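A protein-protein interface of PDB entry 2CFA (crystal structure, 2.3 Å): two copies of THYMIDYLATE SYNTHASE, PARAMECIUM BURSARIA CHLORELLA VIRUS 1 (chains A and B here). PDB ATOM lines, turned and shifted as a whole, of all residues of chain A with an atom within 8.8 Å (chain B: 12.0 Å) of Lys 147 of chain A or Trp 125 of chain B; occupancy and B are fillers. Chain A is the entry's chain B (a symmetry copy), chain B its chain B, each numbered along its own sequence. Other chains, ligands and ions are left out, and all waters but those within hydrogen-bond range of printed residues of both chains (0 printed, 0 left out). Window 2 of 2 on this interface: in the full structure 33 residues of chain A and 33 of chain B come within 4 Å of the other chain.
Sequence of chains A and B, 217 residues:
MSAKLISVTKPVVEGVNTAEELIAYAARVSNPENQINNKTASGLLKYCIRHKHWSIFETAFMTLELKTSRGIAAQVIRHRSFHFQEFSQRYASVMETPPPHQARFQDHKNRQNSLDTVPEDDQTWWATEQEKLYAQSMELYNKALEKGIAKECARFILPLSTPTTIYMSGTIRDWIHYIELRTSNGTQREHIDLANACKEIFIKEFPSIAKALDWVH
No position is printed for both chains. Of the 6 pairs that touch across the chains among the printed residues, none has its exchanged pair printed and touching as well.
Of the 10 printed residues of chain B, 5 touch a printed residue of chain A. Hydrophobic or aromatic side chains of chain B within 4 Å of the printed part of chain A: Trp 125, Trp 126 and Leu 133. Of the 13 printed residues of chain A, 4 touch a printed residue of chain B. Hydrophobic or aromatic side chains of chain A that line the printed part of chain B: Leu 140, Ala 144 and Ile 157.
Of the printed residues of chain B, Lys 147 of chain A touches Trp 125. Trp 125 of chain B touches one residue of chain A. Of the printed residues of chain B, Leu 140 of chain A touches Glu 129 (3.7 Å) and Leu 133 (3.8 Å). No residue of chain B comes within 4 Å of Lys 143 of chain A. Of chain B, only Trp 126 (3.6 Å) comes within 4 Å of Ala 144 of chain A. No residue of chain B comes within 4 Å of Leu 145 of chain A. No residue of chain B comes within 4 Å of Glu 146 of chain A. Gly 148 of chain A touches none of the printed residues of chain B. No residue of chain B comes within 4 Å of Ile 149 of chain A. Of the printed residues of chain A, Glu 129 of chain B touches Leu 140 (3.7 Å). Printed residues of chain A within 4 Å of Gln 130 of chain B: Ile 157. Printed residues of chain B within 4 Å of Ile 157 of chain A: Trp 126 and Gln 130. Of the printed residues of chain A, Leu 133 of chain B touches Leu 140 (3.8 Å). Printed residues of chain A within 4 Å of Trp 126 of chain B: Ala 144 (3.6 Å) and Ile 157 (3.7 Å). Ala 127 of chain B touches none of the printed residues of chain A. Glu 131 of chain B touches none of the printed residues of chain A. The nearest residue of chain B that does not touch Lys 147 of chain A is Trp 126 of chain B (7.6 Å).
CD2 of Leu 140 of chain A touches O of Glu 129 of chain B (3.7 Å). Leu 140 of chain A touches Leu 133 of chain B (CD2 to CD2, 3.8 Å). CZ3 of Trp 126 of chain B touches CB of Ala 144 of chain A, 3.6 Å away. Lys 147 of chain A touches Trp 125 of chain B (CD to CH2, 3.8 Å). Trp 126 of chain B touches Ile 157 of chain A. Gln 130 of chain B touches Ile 157 of chain A.
OE1 of Gln 130 of chain B is in hydrogen-bond range of NE1 of Trp 126 of chain B (3.1 Å). The side-chain carboxylate (OE2) of Glu 129 of chain B is in salt-bridge range of the side-chain amino group (NZ) of Lys 132 of chain B (3.0 Å). O of Ala 144 of chain A is in hydrogen-bond range of N of Ile 149 of chain A, 2.9 Å away.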
ATOM      1  N   GLU A 139      29.584  29.650 -28.696  1.00  0.00           N
ATOM      2  CA  GLU A 139      30.080  28.410 -28.097  1.00  0.00           C
ATOM      3  C   GLU A 139      28.925  27.647 -27.443  1.00  0.00           C
ATOM      4  O   GLU A 139      28.739  26.454 -27.695  1.00  0.00           O
ATOM      5  CB  GLU A 139      31.192  28.715 -27.079  1.00  0.00           C
ATOM      6  CG  GLU A 139      31.676  27.520 -26.237  1.00  0.00           C
ATOM      7  CD  GLU A 139      30.912  27.348 -24.918  1.00  0.00           C
ATOM      8  OE1 GLU A 139      30.360  28.345 -24.397  1.00  0.00           O
ATOM      9  OE2 GLU A 139      30.873  26.208 -24.398  1.00  0.00           O
ATOM     10  N   LEU A 140      28.156  28.354 -26.617  1.00  0.00           N
ATOM     11  CA  LEU A 140      27.005  27.780 -25.927  1.00  0.00           C
ATOM     12  C   LEU A 140      25.903  27.399 -26.912  1.00  0.00           C
ATOM     13  O   LEU A 140      25.213  26.401 -26.715  1.00  0.00           O
ATOM     14  CB  LEU A 140      26.479  28.748 -24.855  1.00  0.00           C
ATOM     15  CG  LEU A 140      25.302  28.358 -23.949  1.00  0.00           C
ATOM     16  CD1 LEU A 140      25.520  27.034 -23.240  1.00  0.00           C
ATOM     17  CD2 LEU A 140      25.028  29.458 -22.940  1.00  0.00           C
ATOM     18  N   TYR A 141      25.757  28.188 -27.975  1.00  0.00           N
ATOM     19  CA  TYR A 141      24.784  27.902 -29.029  1.00  0.00           C
ATOM     20  C   TYR A 141      25.115  26.602 -29.766  1.00  0.00           C
ATOM     21  O   TYR A 141      24.258  25.724 -29.894  1.00  0.00           O
ATOM     22  CB  TYR A 141      24.685  29.074 -30.013  1.00  0.00           C
ATOM     23  CG  TYR A 141      23.817  28.801 -31.226  1.00  0.00           C
ATOM     24  CD1 TYR A 141      22.428  28.705 -31.109  1.00  0.00           C
ATOM     25  CD2 TYR A 141      24.384  28.643 -32.490  1.00  0.00           C
ATOM     26  CE1 TYR A 141      21.626  28.451 -32.221  1.00  0.00           C
ATOM     27  CE2 TYR A 141      23.591  28.390 -33.610  1.00  0.00           C
ATOM     28  CZ  TYR A 141      22.214  28.296 -33.466  1.00  0.00           C
ATOM     29  OH  TYR A 141      21.428  28.048 -34.567  1.00  0.00           O
ATOM     30  N   ASN A 142      26.357  26.490 -30.236  1.00  0.00           N
ATOM     31  CA  ASN A 142      26.818  25.321 -30.990  1.00  0.00           C
ATOM     32  C   ASN A 142      26.804  24.026 -30.183  1.00  0.00           C
ATOM     33  O   ASN A 142      26.562  22.949 -30.735  1.00  0.00           O
ATOM     34  CB  ASN A 142      28.219  25.562 -31.561  1.00  0.00           C
ATOM     35  CG  ASN A 142      28.198  26.357 -32.855  1.00  0.00           C
ATOM     36  OD1 ASN A 142      28.746  27.455 -32.929  1.00  0.00           O
ATOM     37  ND2 ASN A 142      27.566  25.801 -33.886  1.00  0.00           N
ATOM     38  N   LYS A 143      27.063  24.146 -28.883  1.00  0.00           N
ATOM     39  CA  LYS A 143      27.131  22.997 -27.984  1.00  0.00           C
ATOM     40  C   LYS A 143      25.746  22.567 -27.500  1.00  0.00           C
ATOM     41  O   LYS A 143      25.512  21.379 -27.267  1.00  0.00           O
ATOM     42  CB  LYS A 143      28.056  23.296 -26.799  1.00  0.00           C
ATOM     43  CG  LYS A 143      28.622  22.059 -26.101  1.00  0.00           C
ATOM     44  CD  LYS A 143      29.613  22.447 -25.001  1.00  0.00           C
ATOM     45  CE  LYS A 143      30.139  21.229 -24.246  1.00  0.00           C
ATOM     46  NZ  LYS A 143      29.102  20.587 -23.384  1.00  0.00           N
ATOM     47  N   ALA A 144      24.835  23.532 -27.356  1.00  0.00           N
ATOM     48  CA  ALA A 144      23.445  23.243 -26.987  1.00  0.00           C
ATOM     49  C   ALA A 144      22.749  22.406 -28.061  1.00  0.00           C
ATOM     50  O   ALA A 144      22.002  21.479 -27.743  1.00  0.00           O
ATOM     51  CB  ALA A 144      22.677  24.528 -26.730  1.00  0.00           C
ATOM     52  N   LEU A 145      23.006  22.741 -29.325  1.00  0.00           N
ATOM     53  CA  LEU A 145      22.515  21.970 -30.468  1.00  0.00           C
ATOM     54  C   LEU A 145      23.111  20.566 -30.466  1.00  0.00           C
ATOM     55  O   LEU A 145      22.410  19.580 -30.708  1.00  0.00           O
ATOM     56  CB  LEU A 145      22.853  22.680 -31.784  1.00  0.00           C
ATOM     57  CG  LEU A 145      22.186  24.026 -32.098  1.00  0.00           C
ATOM     58  CD1 LEU A 145      22.885  24.711 -33.263  1.00  0.00           C
ATOM     59  CD2 LEU A 145      20.705  23.850 -32.394  1.00  0.00           C
ATOM     60  N   GLU A 146      24.411  20.494 -30.181  1.00  0.00           N
ATOM     61  CA  GLU A 146      25.145  19.233 -30.095  1.00  0.00           C
ATOM     62  C   GLU A 146      24.653  18.374 -28.920  1.00  0.00           C
ATOM     63  O   GLU A 146      24.763  17.147 -28.955  1.00  0.00           O
ATOM     64  CB  GLU A 146      26.654  19.520 -30.001  1.00  0.00           C
ATOM     65  CG  GLU A 146      27.578  18.316 -30.190  1.00  0.00           C
ATOM     66  CD  GLU A 146      28.133  17.783 -28.877  1.00  0.00           C
ATOM     67  OE1 GLU A 146      28.817  18.545 -28.157  1.00  0.00           O
ATOM     68  OE2 GLU A 146      27.896  16.595 -28.571  1.00  0.00           O
ATOM     69  N   LYS A 147      24.098  19.023 -27.897  1.00  0.00           N
ATOM     70  CA  LYS A 147      23.519  18.319 -26.747  1.00  0.00           C
ATOM     71  C   LYS A 147      22.027  17.997 -26.915  1.00  0.00           C
ATOM     72  O   LYS A 147      21.384  17.510 -25.982  1.00  0.00           O
ATOM     73  CB  LYS A 147      23.758  19.097 -25.447  1.00  0.00           C
ATOM     74  CG  LYS A 147      25.202  19.048 -24.943  1.00  0.00           C
ATOM     75  CD  LYS A 147      25.284  19.197 -23.427  1.00  0.00           C
ATOM     76  CE  LYS A 147      25.018  17.871 -22.720  1.00  0.00           C
ATOM     77  NZ  LYS A 147      25.124  17.994 -21.241  1.00  0.00           N
ATOM     78  N   GLY A 148      21.484  18.270 -28.101  1.00  0.00           N
ATOM     79  CA  GLY A 148      20.113  17.876 -28.437  1.00  0.00           C
ATOM     80  C   GLY A 148      19.039  18.948 -28.332  1.00  0.00           C
ATOM     81  O   GLY A 148      17.870  18.686 -28.632  1.00  0.00           O
ATOM     82  N   ILE A 149      19.428  20.150 -27.906  1.00  0.00           N
ATOM     83  CA  ILE A 149      18.497  21.277 -27.787  1.00  0.00           C
ATOM     84  C   ILE A 149      18.143  21.822 -29.171  1.00  0.00           C
ATOM     85  O   ILE A 149      19.023  22.233 -29.933  1.00  0.00           O
ATOM     86  CB  ILE A 149      19.066  22.416 -26.879  1.00  0.00           C
ATOM     87  CG1 ILE A 149      19.315  21.921 -25.441  1.00  0.00           C
ATOM     88  CG2 ILE A 149      18.168  23.660 -26.908  1.00  0.00           C
ATOM     89  CD1 ILE A 149      18.064  21.488 -24.667  1.00  0.00           C
ATOM     90  N   ALA A 150      16.850  21.803 -29.489  1.00  0.00           N
ATOM     91  CA  ALA A 150      16.351  22.296 -30.769  1.00  0.00           C
ATOM     92  C   ALA A 150      15.171  23.231 -30.552  1.00  0.00           C
ATOM     93  O   ALA A 150      15.323  24.303 -29.970  1.00  0.00           O
ATOM     94  CB  ALA A 150      15.957  21.135 -31.680  1.00  0.00           C
ATOM     95  N   ILE A 157      19.343  32.616 -26.881  1.00  0.00           N
ATOM     96  CA  ILE A 157      20.546  33.085 -26.184  1.00  0.00           C
ATOM     97  C   ILE A 157      21.450  33.946 -27.074  1.00  0.00           C
ATOM     98  O   ILE A 157      22.403  34.557 -26.592  1.00  0.00           O
ATOM     99  CB  ILE A 157      21.358  31.911 -25.562  1.00  0.00           C
ATOM    100  CG1 ILE A 157      22.012  31.051 -26.654  1.00  0.00           C
ATOM    101  CG2 ILE A 157      20.471  31.086 -24.629  1.00  0.00           C
ATOM    102  CD1 ILE A 157      23.081  30.088 -26.160  1.00  0.00           C
ATOM    103  N   TRP B 125      20.483  22.076 -16.466  1.00  0.00           N
ATOM    104  CA  TRP B 125      21.736  22.511 -17.075  1.00  0.00           C
ATOM    105  C   TRP B 125      21.524  23.671 -18.046  1.00  0.00           C
ATOM    106  O   TRP B 125      22.268  24.653 -18.021  1.00  0.00           O
ATOM    107  CB  TRP B 125      22.427  21.344 -17.790  1.00  0.00           C
ATOM    108  CG  TRP B 125      23.631  21.761 -18.592  1.00  0.00           C
ATOM    109  CD1 TRP B 125      24.902  21.941 -18.126  1.00  0.00           C
ATOM    110  CD2 TRP B 125      23.671  22.061 -19.995  1.00  0.00           C
ATOM    111  NE1 TRP B 125      25.733  22.330 -19.151  1.00  0.00           N
ATOM    112  CE2 TRP B 125      25.004  22.411 -20.309  1.00  0.00           C
ATOM    113  CE3 TRP B 125      22.711  22.067 -21.017  1.00  0.00           C
ATOM    114  CZ2 TRP B 125      25.402  22.764 -21.604  1.00  0.00           C
ATOM    115  CZ3 TRP B 125      23.109  22.417 -22.307  1.00  0.00           C
ATOM    116  CH2 TRP B 125      24.443  22.760 -22.586  1.00  0.00           C
ATOM    117  N   TRP B 126      20.519  23.539 -18.912  1.00  0.00           N
ATOM    118  CA  TRP B 126      20.180  24.581 -19.880  1.00  0.00           C
ATOM    119  C   TRP B 126      19.733  25.848 -19.153  1.00  0.00           C
ATOM    120  O   TRP B 126      20.194  26.945 -19.469  1.00  0.00           O
ATOM    121  CB  TRP B 126      19.107  24.079 -20.857  1.00  0.00           C
ATOM    122  CG  TRP B 126      18.693  25.068 -21.932  1.00  0.00           C
ATOM    123  CD1 TRP B 126      17.419  25.464 -22.229  1.00  0.00           C
ATOM    124  CD2 TRP B 126      19.553  25.772 -22.845  1.00  0.00           C
ATOM    125  NE1 TRP B 126      17.430  26.366 -23.265  1.00  0.00           N
ATOM    126  CE2 TRP B 126      18.724  26.576 -23.661  1.00  0.00           C
ATOM    127  CE3 TRP B 126      20.940  25.805 -23.051  1.00  0.00           C
ATOM    128  CZ2 TRP B 126      19.237  27.402 -24.666  1.00  0.00           C
ATOM    129  CZ3 TRP B 126      21.448  26.627 -24.049  1.00  0.00           C
ATOM    130  CH2 TRP B 126      20.597  27.413 -24.845  1.00  0.00           C
ATOM    131  N   ALA B 127      18.862  25.678 -18.159  1.00  0.00           N
ATOM    132  CA  ALA B 127      18.411  26.777 -17.305  1.00  0.00           C
ATOM    133  C   ALA B 127      19.520  27.294 -16.379  1.00  0.00           C
ATOM    134  O   ALA B 127      19.340  28.302 -15.693  1.00  0.00           O
ATOM    135  CB  ALA B 127      17.194  26.346 -16.494  1.00  0.00           C
ATOM    136  N   THR B 128      20.657  26.596 -16.363  1.00  0.00           N
ATOM    137  CA  THR B 128      21.815  26.991 -15.555  1.00  0.00           C
ATOM    138  C   THR B 128      22.811  27.800 -16.390  1.00  0.00           C
ATOM    139  O   THR B 128      23.241  28.875 -15.974  1.00  0.00           O
ATOM    140  CB  THR B 128      22.523  25.763 -14.918  1.00  0.00           C
ATOM    141  OG1 THR B 128      21.546  24.877 -14.355  1.00  0.00           O
ATOM    142  CG2 THR B 128      23.503  26.195 -13.827  1.00  0.00           C
ATOM    143  N   GLU B 129      23.162  27.278 -17.565  1.00  0.00           N
ATOM    144  CA  GLU B 129      24.098  27.939 -18.479  1.00  0.00           C
ATOM    145  C   GLU B 129      23.517  29.220 -19.085  1.00  0.00           C
ATOM    146  O   GLU B 129      24.256  30.163 -19.380  1.00  0.00           O
ATOM    147  CB  GLU B 129      24.536  26.984 -19.594  1.00  0.00           C
ATOM    148  CG  GLU B 129      25.305  25.753 -19.121  1.00  0.00           C
ATOM    149  CD  GLU B 129      26.705  26.068 -18.613  1.00  0.00           C
ATOM    150  OE1 GLU B 129      27.405  26.896 -19.237  1.00  0.00           O
ATOM    151  OE2 GLU B 129      27.110  25.476 -17.589  1.00  0.00           O
ATOM    152  N   GLN B 130      22.198  29.237 -19.274  1.00  0.00           N
ATOM    153  CA  GLN B 130      21.477  30.432 -19.712  1.00  0.00           C
ATOM    154  C   GLN B 130      21.551  31.530 -18.661  1.00  0.00           C
ATOM    155  O   GLN B 130      21.820  32.685 -18.986  1.00  0.00           O
ATOM    156  CB  GLN B 130      20.010  30.110 -19.988  1.00  0.00           C
ATOM    157  CG  GLN B 130      19.721  29.552 -21.363  1.00  0.00           C
ATOM    158  CD  GLN B 130      18.233  29.382 -21.600  1.00  0.00           C
ATOM    159  OE1 GLN B 130      17.592  28.514 -21.004  1.00  0.00           O
ATOM    160  NE2 GLN B 130      17.674  30.213 -22.474  1.00  0.00           N
ATOM    161  N   GLU B 131      21.304  31.156 -17.406  1.00  0.00           N
ATOM    162  CA  GLU B 131      21.331  32.091 -16.280  1.00  0.00           C
ATOM    163  C   GLU B 131      22.717  32.670 -16.003  1.00  0.00           C
ATOM    164  O   GLU B 131      22.828  33.816 -15.562  1.00  0.00           O
ATOM    165  CB  GLU B 131      20.756  31.440 -15.019  1.00  0.00           C
ATOM    166  CG  GLU B 131      19.375  31.959 -14.606  1.00  0.00           C
ATOM    167  CD  GLU B 131      18.341  31.922 -15.727  1.00  0.00           C
ATOM    168  OE1 GLU B 131      17.735  32.980 -16.008  1.00  0.00           O
ATOM    169  OE2 GLU B 131      18.130  30.843 -16.325  1.00  0.00           O
ATOM    170  N   LYS B 132      23.762  31.885 -16.260  1.00  0.00           N
ATOM    171  CA  LYS B 132      25.135  32.378 -16.155  1.00  0.00           C
ATOM    172  C   LYS B 132      25.444  33.384 -17.259  1.00  0.00           C
ATOM    173  O   LYS B 132      26.074  34.413 -17.004  1.00  0.00           O
ATOM    174  CB  LYS B 132      26.156  31.234 -16.182  1.00  0.00           C
ATOM    175  CG  LYS B 132      26.637  30.785 -14.804  1.00  0.00           C
ATOM    176  CD  LYS B 132      26.006  29.464 -14.371  1.00  0.00           C
ATOM    177  CE  LYS B 132      26.936  28.271 -14.610  1.00  0.00           C
ATOM    178  NZ  LYS B 132      27.322  28.073 -16.040  1.00  0.00           N
ATOM    179  N   LEU B 133      24.993  33.081 -18.477  1.00  0.00           N
ATOM    180  CA  LEU B 133      25.228  33.944 -19.635  1.00  0.00           C
ATOM    181  C   LEU B 133      24.367  35.209 -19.607  1.00  0.00           C
ATOM    182  O   LEU B 133      24.849  36.294 -19.947  1.00  0.00           O
ATOM    183  CB  LEU B 133      25.014  33.175 -20.945  1.00  0.00           C
ATOM    184  CG  LEU B 133      25.547  33.813 -22.234  1.00  0.00           C
ATOM    185  CD1 LEU B 133      27.047  33.598 -22.387  1.00  0.00           C
ATOM    186  CD2 LEU B 133      24.812  33.264 -23.445  1.00  0.00           C
ATOM    187  N   TYR B 134      23.103  35.066 -19.200  1.00  0.00           N
ATOM    188  CA  TYR B 134      22.181  36.200 -19.101  1.00  0.00           C
ATOM    189  C   TYR B 134      22.650  37.213 -18.059  1.00  0.00           C
ATOM    190  O   TYR B 134      22.612  38.421 -18.304  1.00  0.00           O
ATOM    191  CB  TYR B 134      20.748  35.739 -18.799  1.00  0.00           C
ATOM    192  CG  TYR B 134      19.726  36.864 -18.818  1.00  0.00           C
ATOM    193  CD1 TYR B 134      19.223  37.356 -20.024  1.00  0.00           C
ATOM    194  CD2 TYR B 134      19.265  37.438 -17.631  1.00  0.00           C
ATOM    195  CE1 TYR B 134      18.287  38.394 -20.050  1.00  0.00           C
ATOM    196  CE2 TYR B 134      18.328  38.474 -17.644  1.00  0.00           C
ATOM    197  CZ  TYR B 134      17.844  38.946 -18.857  1.00  0.00           C
ATOM    198  OH  TYR B 134      16.921  39.969 -18.879  1.00  0.00           O
